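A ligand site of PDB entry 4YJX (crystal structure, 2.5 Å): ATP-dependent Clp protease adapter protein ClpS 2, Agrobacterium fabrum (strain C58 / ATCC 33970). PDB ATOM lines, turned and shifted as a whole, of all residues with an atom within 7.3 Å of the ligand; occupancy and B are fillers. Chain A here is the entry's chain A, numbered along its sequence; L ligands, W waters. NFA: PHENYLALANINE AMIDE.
OG1 of Thr 34 sits at hydrogen-bond distance from N of Leu 95.
The side-chain carboxylate (OD1) of Asp 31 is in hydrogen-bond range of the backbone NH (N) of Tyr 33 (2.7 Å).
The backbone NH (N) of Asn 30 is in hydrogen-bond range of the backbone carbonyl oxygen (O) of Gly 65 (3.0 Å).
N of Leu 29 sits at hydrogen-bond distance from O of Met 96, at 3.1 Å.
O of Arg 36 is in hydrogen-bond range of OG1 of Thr 40, at 3.1 Å.
The backbone NH (N) of Thr 34 is in hydrogen-bond range of the side-chain carboxylate (OD1) of Asp 31 (2.7 Å).
Water W1 lies within hydrogen-bond range of the side-chain carboxylate of Asp 32, a nitrogen (N) of the ligand, the backbone carbonyl oxygen of Asp 31 and the side-chain amide nitrogen of Asn 30.
A ring nitrogen (ND1) of His 62 lies within hydrogen-bond range of a nitrogen (N) of the ligand, 2.9 Å away.
A nitrogen (N) of the ligand lies within hydrogen-bond range of the side-chain amide oxygen of Asn 30 (3.1 Å).
A nitrogen (N) of the ligand is in hydrogen-bond range of the backbone carbonyl oxygen of Asp 31, 3.1 Å away.
NXT of the ligand sits at hydrogen-bond distance from O of Thr 34, at 2.6 Å.
Leu 28 touches the ligand.
Leu 29 touches the ligand (O to CZ, 3.4 Å).
Pro 35 touches the ligand (CA to NXT, 3.9 Å).
Arg 36 touches the ligand.
Val 39 touches the ligand (CG2 to CE1, 3.8 Å).
Met 58 touches the ligand.
Ala 61 touches the ligand (CB to CE2, 3.97 Å).
Hydrophobic or aromatic side chains that line the ligand: Leu 28, Val 39, Met 58, Ala 61 and His 62.
11 residues have an atom within 4 Å of the ligand: Leu 28, Leu 29, Asn 30, Asp 31, Thr 34, Pro 35, Arg 36, Val 39, Met 58, Ala 61 and His 62.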
ATOM      1  N   LEU A  28      20.932 -31.614  18.633  1.00  0.00           N
ATOM      2  CA  LEU A  28      20.055 -30.478  18.928  1.00  0.00           C
ATOM      3  C   LEU A  28      20.911 -29.227  19.054  1.00  0.00           C
ATOM      4  O   LEU A  28      21.866 -29.209  19.830  1.00  0.00           O
ATOM      5  CB  LEU A  28      19.264 -30.713  20.213  1.00  0.00           C
ATOM      6  CG  LEU A  28      18.567 -29.479  20.818  1.00  0.00           C
ATOM      7  CD1 LEU A  28      17.502 -28.937  19.879  1.00  0.00           C
ATOM      8  CD2 LEU A  28      17.974 -29.794  22.181  1.00  0.00           C
ATOM      9  N   LEU A  29      20.580 -28.191  18.291  1.00  0.00           N
ATOM     10  CA  LEU A  29      21.304 -26.934  18.342  1.00  0.00           C
ATOM     11  C   LEU A  29      20.511 -25.902  19.133  1.00  0.00           C
ATOM     12  O   LEU A  29      19.292 -25.829  19.026  1.00  0.00           O
ATOM     13  CB  LEU A  29      21.570 -26.410  16.936  1.00  0.00           C
ATOM     14  CG  LEU A  29      22.213 -27.387  15.958  1.00  0.00           C
ATOM     15  CD1 LEU A  29      22.584 -26.656  14.689  1.00  0.00           C
ATOM     16  CD2 LEU A  29      23.431 -28.047  16.584  1.00  0.00           C
ATOM     17  N   ASN A  30      21.229 -25.102  19.914  1.00  0.00           N
ATOM     18  CA  ASN A  30      20.600 -24.017  20.653  1.00  0.00           C
ATOM     19  C   ASN A  30      20.202 -22.867  19.745  1.00  0.00           C
ATOM     20  O   ASN A  30      20.766 -22.677  18.679  1.00  0.00           O
ATOM     21  CB  ASN A  30      21.522 -23.502  21.751  1.00  0.00           C
ATOM     22  CG  ASN A  30      20.818 -22.540  22.693  1.00  0.00           C
ATOM     23  OD1 ASN A  30      19.739 -22.831  23.193  1.00  0.00           O
ATOM     24  ND2 ASN A  30      21.427 -21.379  22.914  1.00  0.00           N
ATOM     25  N   ASP A  31      19.205 -22.114  20.183  1.00  0.00           N
ATOM     26  CA  ASP A  31      18.860 -20.851  19.574  1.00  0.00           C
ATOM     27  C   ASP A  31      18.192 -20.010  20.654  1.00  0.00           C
ATOM     28  O   ASP A  31      17.893 -20.517  21.737  1.00  0.00           O
ATOM     29  CB  ASP A  31      17.958 -21.031  18.344  1.00  0.00           C
ATOM     30  CG  ASP A  31      16.530 -21.443  18.700  1.00  0.00           C
ATOM     31  OD1 ASP A  31      15.760 -20.579  19.175  1.00  0.00           O
ATOM     32  OD2 ASP A  31      16.178 -22.612  18.466  1.00  0.00           O
ATOM     33  N   ASP A  32      17.974 -18.730  20.393  1.00  0.00           N
ATOM     34  CA  ASP A  32      17.457 -17.830  21.414  1.00  0.00           C
ATOM     35  C   ASP A  32      15.946 -17.629  21.381  1.00  0.00           C
ATOM     36  O   ASP A  32      15.414 -16.901  22.210  1.00  0.00           O
ATOM     37  CB  ASP A  32      18.128 -16.452  21.277  1.00  0.00           C
ATOM     38  CG  ASP A  32      19.556 -16.455  21.784  1.00  0.00           C
ATOM     39  OD1 ASP A  32      19.926 -17.380  22.536  1.00  0.00           O
ATOM     40  OD2 ASP A  32      20.311 -15.517  21.447  1.00  0.00           O
ATOM     41  N   TYR A  33      15.239 -18.281  20.458  1.00  0.00           N
ATOM     42  CA  TYR A  33      13.825 -17.965  20.243  1.00  0.00           C
ATOM     43  C   TYR A  33      12.871 -19.111  20.580  1.00  0.00           C
ATOM     44  O   TYR A  33      11.777 -18.878  21.089  1.00  0.00           O
ATOM     45  CB  TYR A  33      13.617 -17.526  18.793  1.00  0.00           C
ATOM     46  CG  TYR A  33      14.501 -16.354  18.410  1.00  0.00           C
ATOM     47  CD1 TYR A  33      14.038 -15.049  18.517  1.00  0.00           C
ATOM     48  CD2 TYR A  33      15.788 -16.562  17.963  1.00  0.00           C
ATOM     49  CE1 TYR A  33      14.850 -13.975  18.174  1.00  0.00           C
ATOM     50  CE2 TYR A  33      16.606 -15.500  17.625  1.00  0.00           C
ATOM     51  CZ  TYR A  33      16.132 -14.217  17.730  1.00  0.00           C
ATOM     52  OH  TYR A  33      16.956 -13.163  17.388  1.00  0.00           O
ATOM     53  N   THR A  34      13.274 -20.344  20.314  1.00  0.00           N
ATOM     54  CA  THR A  34      12.417 -21.492  20.572  1.00  0.00           C
ATOM     55  C   THR A  34      12.201 -21.650  22.080  1.00  0.00           C
ATOM     56  O   THR A  34      13.175 -21.689  22.833  1.00  0.00           O
ATOM     57  CB  THR A  34      13.025 -22.798  20.011  1.00  0.00           C
ATOM     58  OG1 THR A  34      13.394 -22.622  18.641  1.00  0.00           O
ATOM     59  CG2 THR A  34      12.019 -23.937  20.113  1.00  0.00           C
ATOM     60  N   PRO A  35      10.938 -21.732  22.523  1.00  0.00           N
ATOM     61  CA  PRO A  35      10.687 -21.947  23.958  1.00  0.00           C
ATOM     62  C   PRO A  35      11.320 -23.226  24.491  1.00  0.00           C
ATOM     63  O   PRO A  35      11.314 -24.253  23.799  1.00  0.00           O
ATOM     64  CB  PRO A  35       9.155 -22.036  24.026  1.00  0.00           C
ATOM     65  CG  PRO A  35       8.684 -21.264  22.852  1.00  0.00           C
ATOM     66  CD  PRO A  35       9.696 -21.492  21.774  1.00  0.00           C
ATOM     67  N   ARG A  36      11.842 -23.172  25.714  1.00  0.00           N
ATOM     68  CA  ARG A  36      12.485 -24.325  26.340  1.00  0.00           C
ATOM     69  C   ARG A  36      11.550 -25.537  26.376  1.00  0.00           C
ATOM     70  O   ARG A  36      11.950 -26.634  26.017  1.00  0.00           O
ATOM     71  CB  ARG A  36      12.944 -23.969  27.760  1.00  0.00           C
ATOM     72  CG  ARG A  36      13.969 -22.843  27.805  1.00  0.00           C
ATOM     73  CD  ARG A  36      14.487 -22.562  29.218  1.00  0.00           C
ATOM     74  NE  ARG A  36      13.409 -22.266  30.157  1.00  0.00           N
ATOM     75  CZ  ARG A  36      12.752 -21.116  30.203  1.00  0.00           C
ATOM     76  NH1 ARG A  36      13.041 -20.131  29.360  1.00  0.00           N
ATOM     77  NH2 ARG A  36      11.780 -20.945  31.093  1.00  0.00           N
ATOM     78  N   GLU A  37      10.306 -25.325  26.803  1.00  0.00           N
ATOM     79  CA  GLU A  37       9.377 -26.438  26.949  1.00  0.00           C
ATOM     80  C   GLU A  37       8.946 -26.999  25.602  1.00  0.00           C
ATOM     81  O   GLU A  37       8.687 -28.194  25.475  1.00  0.00           O
ATOM     82  CB  GLU A  37       8.150 -26.003  27.754  1.00  0.00           C
ATOM     83  CG  GLU A  37       7.202 -27.156  28.087  1.00  0.00           C
ATOM     84  CD  GLU A  37       7.867 -28.235  28.937  1.00  0.00           C
ATOM     85  OE1 GLU A  37       8.852 -27.933  29.633  1.00  0.00           O
ATOM     86  OE2 GLU A  37       7.403 -29.398  28.901  1.00  0.00           O
ATOM     87  N   VAL A  39      10.893 -27.254  22.942  1.00  0.00           N
ATOM     88  CA  VAL A  39      11.996 -28.126  22.564  1.00  0.00           C
ATOM     89  C   VAL A  39      11.800 -29.473  23.256  1.00  0.00           C
ATOM     90  O   VAL A  39      11.958 -30.533  22.658  1.00  0.00           O
ATOM     91  CB  VAL A  39      13.362 -27.511  22.947  1.00  0.00           C
ATOM     92  CG1 VAL A  39      14.510 -28.493  22.704  1.00  0.00           C
ATOM     93  CG2 VAL A  39      13.602 -26.221  22.175  1.00  0.00           C
ATOM     94  N   THR A  40      11.416 -29.406  24.529  1.00  0.00           N
ATOM     95  CA  THR A  40      11.252 -30.593  25.358  1.00  0.00           C
ATOM     96  C   THR A  40      10.190 -31.542  24.807  1.00  0.00           C
ATOM     97  O   THR A  40      10.433 -32.746  24.703  1.00  0.00           O
ATOM     98  CB  THR A  40      10.906 -30.212  26.807  1.00  0.00           C
ATOM     99  OG1 THR A  40      11.963 -29.421  27.353  1.00  0.00           O
ATOM    100  CG2 THR A  40      10.700 -31.448  27.686  1.00  0.00           C
ATOM    101  N   LEU A  43      11.242 -33.271  21.784  1.00  0.00           N
ATOM    102  CA  LEU A  43      12.131 -34.374  22.112  1.00  0.00           C
ATOM    103  C   LEU A  43      11.324 -35.588  22.604  1.00  0.00           C
ATOM    104  O   LEU A  43      11.654 -36.724  22.287  1.00  0.00           O
ATOM    105  CB  LEU A  43      13.168 -33.933  23.158  1.00  0.00           C
ATOM    106  CG  LEU A  43      14.274 -32.996  22.664  1.00  0.00           C
ATOM    107  CD1 LEU A  43      15.052 -32.419  23.840  1.00  0.00           C
ATOM    108  CD2 LEU A  43      15.234 -33.702  21.697  1.00  0.00           C
ATOM    109  N   VAL A  57      18.325 -32.855  28.035  1.00  0.00           N
ATOM    110  CA  VAL A  57      18.933 -32.721  26.712  1.00  0.00           C
ATOM    111  C   VAL A  57      18.734 -31.299  26.210  1.00  0.00           C
ATOM    112  O   VAL A  57      19.675 -30.670  25.714  1.00  0.00           O
ATOM    113  CB  VAL A  57      18.352 -33.719  25.709  1.00  0.00           C
ATOM    114  CG1 VAL A  57      18.903 -33.470  24.301  1.00  0.00           C
ATOM    115  CG2 VAL A  57      18.686 -35.126  26.133  1.00  0.00           C
ATOM    116  N   MET A  58      17.517 -30.797  26.349  1.00  0.00           N
ATOM    117  CA  MET A  58      17.203 -29.414  25.994  1.00  0.00           C
ATOM    118  C   MET A  58      18.132 -28.451  26.723  1.00  0.00           C
ATOM    119  O   MET A  58      18.667 -27.516  26.123  1.00  0.00           O
ATOM    120  CB  MET A  58      15.744 -29.095  26.346  1.00  0.00           C
ATOM    121  CG  MET A  58      15.321 -27.659  26.088  1.00  0.00           C
ATOM    122  SD  MET A  58      15.706 -26.505  27.426  1.00  0.00           S
ATOM    123  CE  MET A  58      14.744 -27.190  28.773  1.00  0.00           C
ATOM    124  N   MET A  59      18.324 -28.686  28.017  1.00  0.00           N
ATOM    125  CA  MET A  59      19.151 -27.797  28.824  1.00  0.00           C
ATOM    126  C   MET A  59      20.626 -27.936  28.479  1.00  0.00           C
ATOM    127  O   MET A  59      21.397 -26.987  28.612  1.00  0.00           O
ATOM    128  CB  MET A  59      18.931 -28.060  30.313  1.00  0.00           C
ATOM    129  CG  MET A  59      17.690 -27.379  30.870  1.00  0.00           C
ATOM    130  SD  MET A  59      17.676 -25.588  30.587  1.00  0.00           S
ATOM    131  CE  MET A  59      19.142 -25.061  31.464  1.00  0.00           C
ATOM    132  N   THR A  60      21.029 -29.121  28.030  1.00  0.00           N
ATOM    133  CA  THR A  60      22.404 -29.334  27.645  1.00  0.00           C
ATOM    134  C   THR A  60      22.729 -28.463  26.437  1.00  0.00           C
ATOM    135  O   THR A  60      23.744 -27.778  26.418  1.00  0.00           O
ATOM    136  CB  THR A  60      22.678 -30.818  27.332  1.00  0.00           C
ATOM    137  OG1 THR A  60      22.460 -31.597  28.509  1.00  0.00           O
ATOM    138  CG2 THR A  60      24.116 -31.017  26.864  1.00  0.00           C
ATOM    139  N   ALA A  61      21.845 -28.469  25.449  1.00  0.00           N
ATOM    140  CA  ALA A  61      22.023 -27.625  24.275  1.00  0.00           C
ATOM    141  C   ALA A  61      21.938 -26.154  24.685  1.00  0.00           C
ATOM    142  O   ALA A  61      22.733 -25.334  24.241  1.00  0.00           O
ATOM    143  CB  ALA A  61      20.977 -27.942  23.223  1.00  0.00           C
ATOM    144  N   HIS A  62      20.985 -25.859  25.560  1.00  0.00           N
ATOM    145  CA  HIS A  62      20.778 -24.503  26.069  1.00  0.00           C
ATOM    146  C   HIS A  62      22.051 -23.892  26.645  1.00  0.00           C
ATOM    147  O   HIS A  62      22.339 -22.721  26.415  1.00  0.00           O
ATOM    148  CB  HIS A  62      19.682 -24.525  27.138  1.00  0.00           C
ATOM    149  CG  HIS A  62      19.483 -23.208  27.824  1.00  0.00           C
ATOM    150  ND1 HIS A  62      18.804 -22.153  27.241  1.00  0.00           N
ATOM    151  CD2 HIS A  62      19.844 -22.783  29.058  1.00  0.00           C
ATOM    152  CE1 HIS A  62      18.778 -21.142  28.088  1.00  0.00           C
ATOM    153  NE2 HIS A  62      19.402 -21.492  29.193  1.00  0.00           N
ATOM    154  N   ARG A  63      22.825 -24.703  27.362  1.00  0.00           N
ATOM    155  CA  ARG A  63      24.025 -24.225  28.063  1.00  0.00           C
ATOM    156  C   ARG A  63      25.288 -24.252  27.220  1.00  0.00           C
ATOM    157  O   ARG A  63      26.104 -23.319  27.298  1.00  0.00           O
ATOM    158  CB  ARG A  63      24.261 -25.060  29.325  1.00  0.00           C
ATOM    159  CG  ARG A  63      23.234 -24.840  30.421  1.00  0.00           C
ATOM    160  CD  ARG A  63      23.560 -25.644  31.660  1.00  0.00           C
ATOM    161  NE  ARG A  63      22.509 -25.549  32.665  1.00  0.00           N
ATOM    162  CZ  ARG A  63      22.342 -24.516  33.493  1.00  0.00           C
ATOM    163  NH1 ARG A  63      23.176 -23.481  33.446  1.00  0.00           N
ATOM    164  NH2 ARG A  63      21.346 -24.530  34.372  1.00  0.00           N
ATOM    165  N   GLY A  65      25.479 -24.896  23.741  1.00  0.00           N
ATOM    166  CA  GLY A  65      25.294 -24.628  22.326  1.00  0.00           C
ATOM    167  C   GLY A  65      24.711 -25.789  21.552  1.00  0.00           C
ATOM    168  O   GLY A  65      24.096 -25.583  20.510  1.00  0.00           O
ATOM    169  N   PRO A  94      13.167 -21.036  14.990  1.00  0.00           N
ATOM    170  CA  PRO A  94      14.393 -21.413  14.281  1.00  0.00           C
ATOM    171  C   PRO A  94      14.980 -22.739  14.782  1.00  0.00           C
ATOM    172  O   PRO A  94      16.129 -23.041  14.470  1.00  0.00           O
ATOM    173  CB  PRO A  94      15.330 -20.236  14.578  1.00  0.00           C
ATOM    174  CG  PRO A  94      14.904 -19.747  15.924  1.00  0.00           C
ATOM    175  CD  PRO A  94      13.423 -20.013  16.026  1.00  0.00           C
ATOM    176  N   LEU A  95      14.201 -23.503  15.546  1.00  0.00           N
ATOM    177  CA  LEU A  95      14.671 -24.772  16.100  1.00  0.00           C
ATOM    178  C   LEU A  95      15.319 -25.655  15.040  1.00  0.00           C
ATOM    179  O   LEU A  95      14.723 -25.944  13.996  1.00  0.00           O
ATOM    180  CB  LEU A  95      13.529 -25.535  16.761  1.00  0.00           C
ATOM    181  CG  LEU A  95      13.913 -26.873  17.409  1.00  0.00           C
ATOM    182  CD1 LEU A  95      14.945 -26.698  18.513  1.00  0.00           C
ATOM    183  CD2 LEU A  95      12.690 -27.573  17.939  1.00  0.00           C
ATOM    184  N   MET A  96      16.543 -26.094  15.319  1.00  0.00           N
ATOM    185  CA  MET A  96      17.307 -26.862  14.349  1.00  0.00           C
ATOM    186  C   MET A  96      17.837 -28.163  14.922  1.00  0.00           C
ATOM    187  O   MET A  96      18.542 -28.168  15.941  1.00  0.00           O
ATOM    188  CB  MET A  96      18.474 -26.025  13.819  1.00  0.00           C
ATOM    189  CG  MET A  96      19.211 -26.686  12.678  1.00  0.00           C
ATOM    190  SD  MET A  96      18.166 -27.030  11.255  1.00  0.00           S
ATOM    191  CE  MET A  96      17.406 -25.422  11.003  1.00  0.00           C
ATOM    192  N   PHE A  97      17.484 -29.266  14.280  1.00  0.00           N
ATOM    193  CA  PHE A  97      18.118 -30.549  14.528  1.00  0.00           C
ATOM    194  C   PHE A  97      18.945 -30.902  13.301  1.00  0.00           C
ATOM    195  O   PHE A  97      18.449 -30.861  12.176  1.00  0.00           O
ATOM    196  CB  PHE A  97      17.088 -31.652  14.780  1.00  0.00           C
ATOM    197  CG  PHE A  97      16.441 -31.596  16.138  1.00  0.00           C
ATOM    198  CD1 PHE A  97      16.815 -32.480  17.141  1.00  0.00           C
ATOM    199  CD2 PHE A  97      15.450 -30.672  16.412  1.00  0.00           C
ATOM    200  CE1 PHE A  97      16.217 -32.438  18.374  1.00  0.00           C
ATOM    201  CE2 PHE A  97      14.845 -30.629  17.658  1.00  0.00           C
ATOM    202  CZ  PHE A  97      15.218 -31.514  18.637  1.00  0.00           C
HETATM  203  N   NFA L   1      17.637 -21.210  24.799  1.00  0.00           N
HETATM  204  CA  NFA L   1      16.273 -21.323  24.389  1.00  0.00           C
HETATM  205  C   NFA L   1      15.422 -20.331  25.140  1.00  0.00           C
HETATM  206  O   NFA L   1      15.896 -19.650  26.021  1.00  0.00           O
HETATM  207  CB  NFA L   1      15.805 -22.731  24.671  1.00  0.00           C
HETATM  208  CG  NFA L   1      16.392 -23.746  23.701  1.00  0.00           C
HETATM  209  CD1 NFA L   1      16.300 -23.547  22.367  1.00  0.00           C
HETATM  210  CD2 NFA L   1      17.062 -25.009  24.212  1.00  0.00           C
HETATM  211  CE1 NFA L   1      16.889 -24.550  21.405  1.00  0.00           C
HETATM  212  CE2 NFA L   1      17.573 -25.900  23.339  1.00  0.00           C
HETATM  213  CZ  NFA L   1      17.487 -25.664  21.851  1.00  0.00           C
HETATM  214  NXT NFA L   1      14.044 -20.198  24.801  1.00  0.00           N
HETATM  215  O   HOH W   1      19.338 -19.075  24.393  1.00  0.00           O
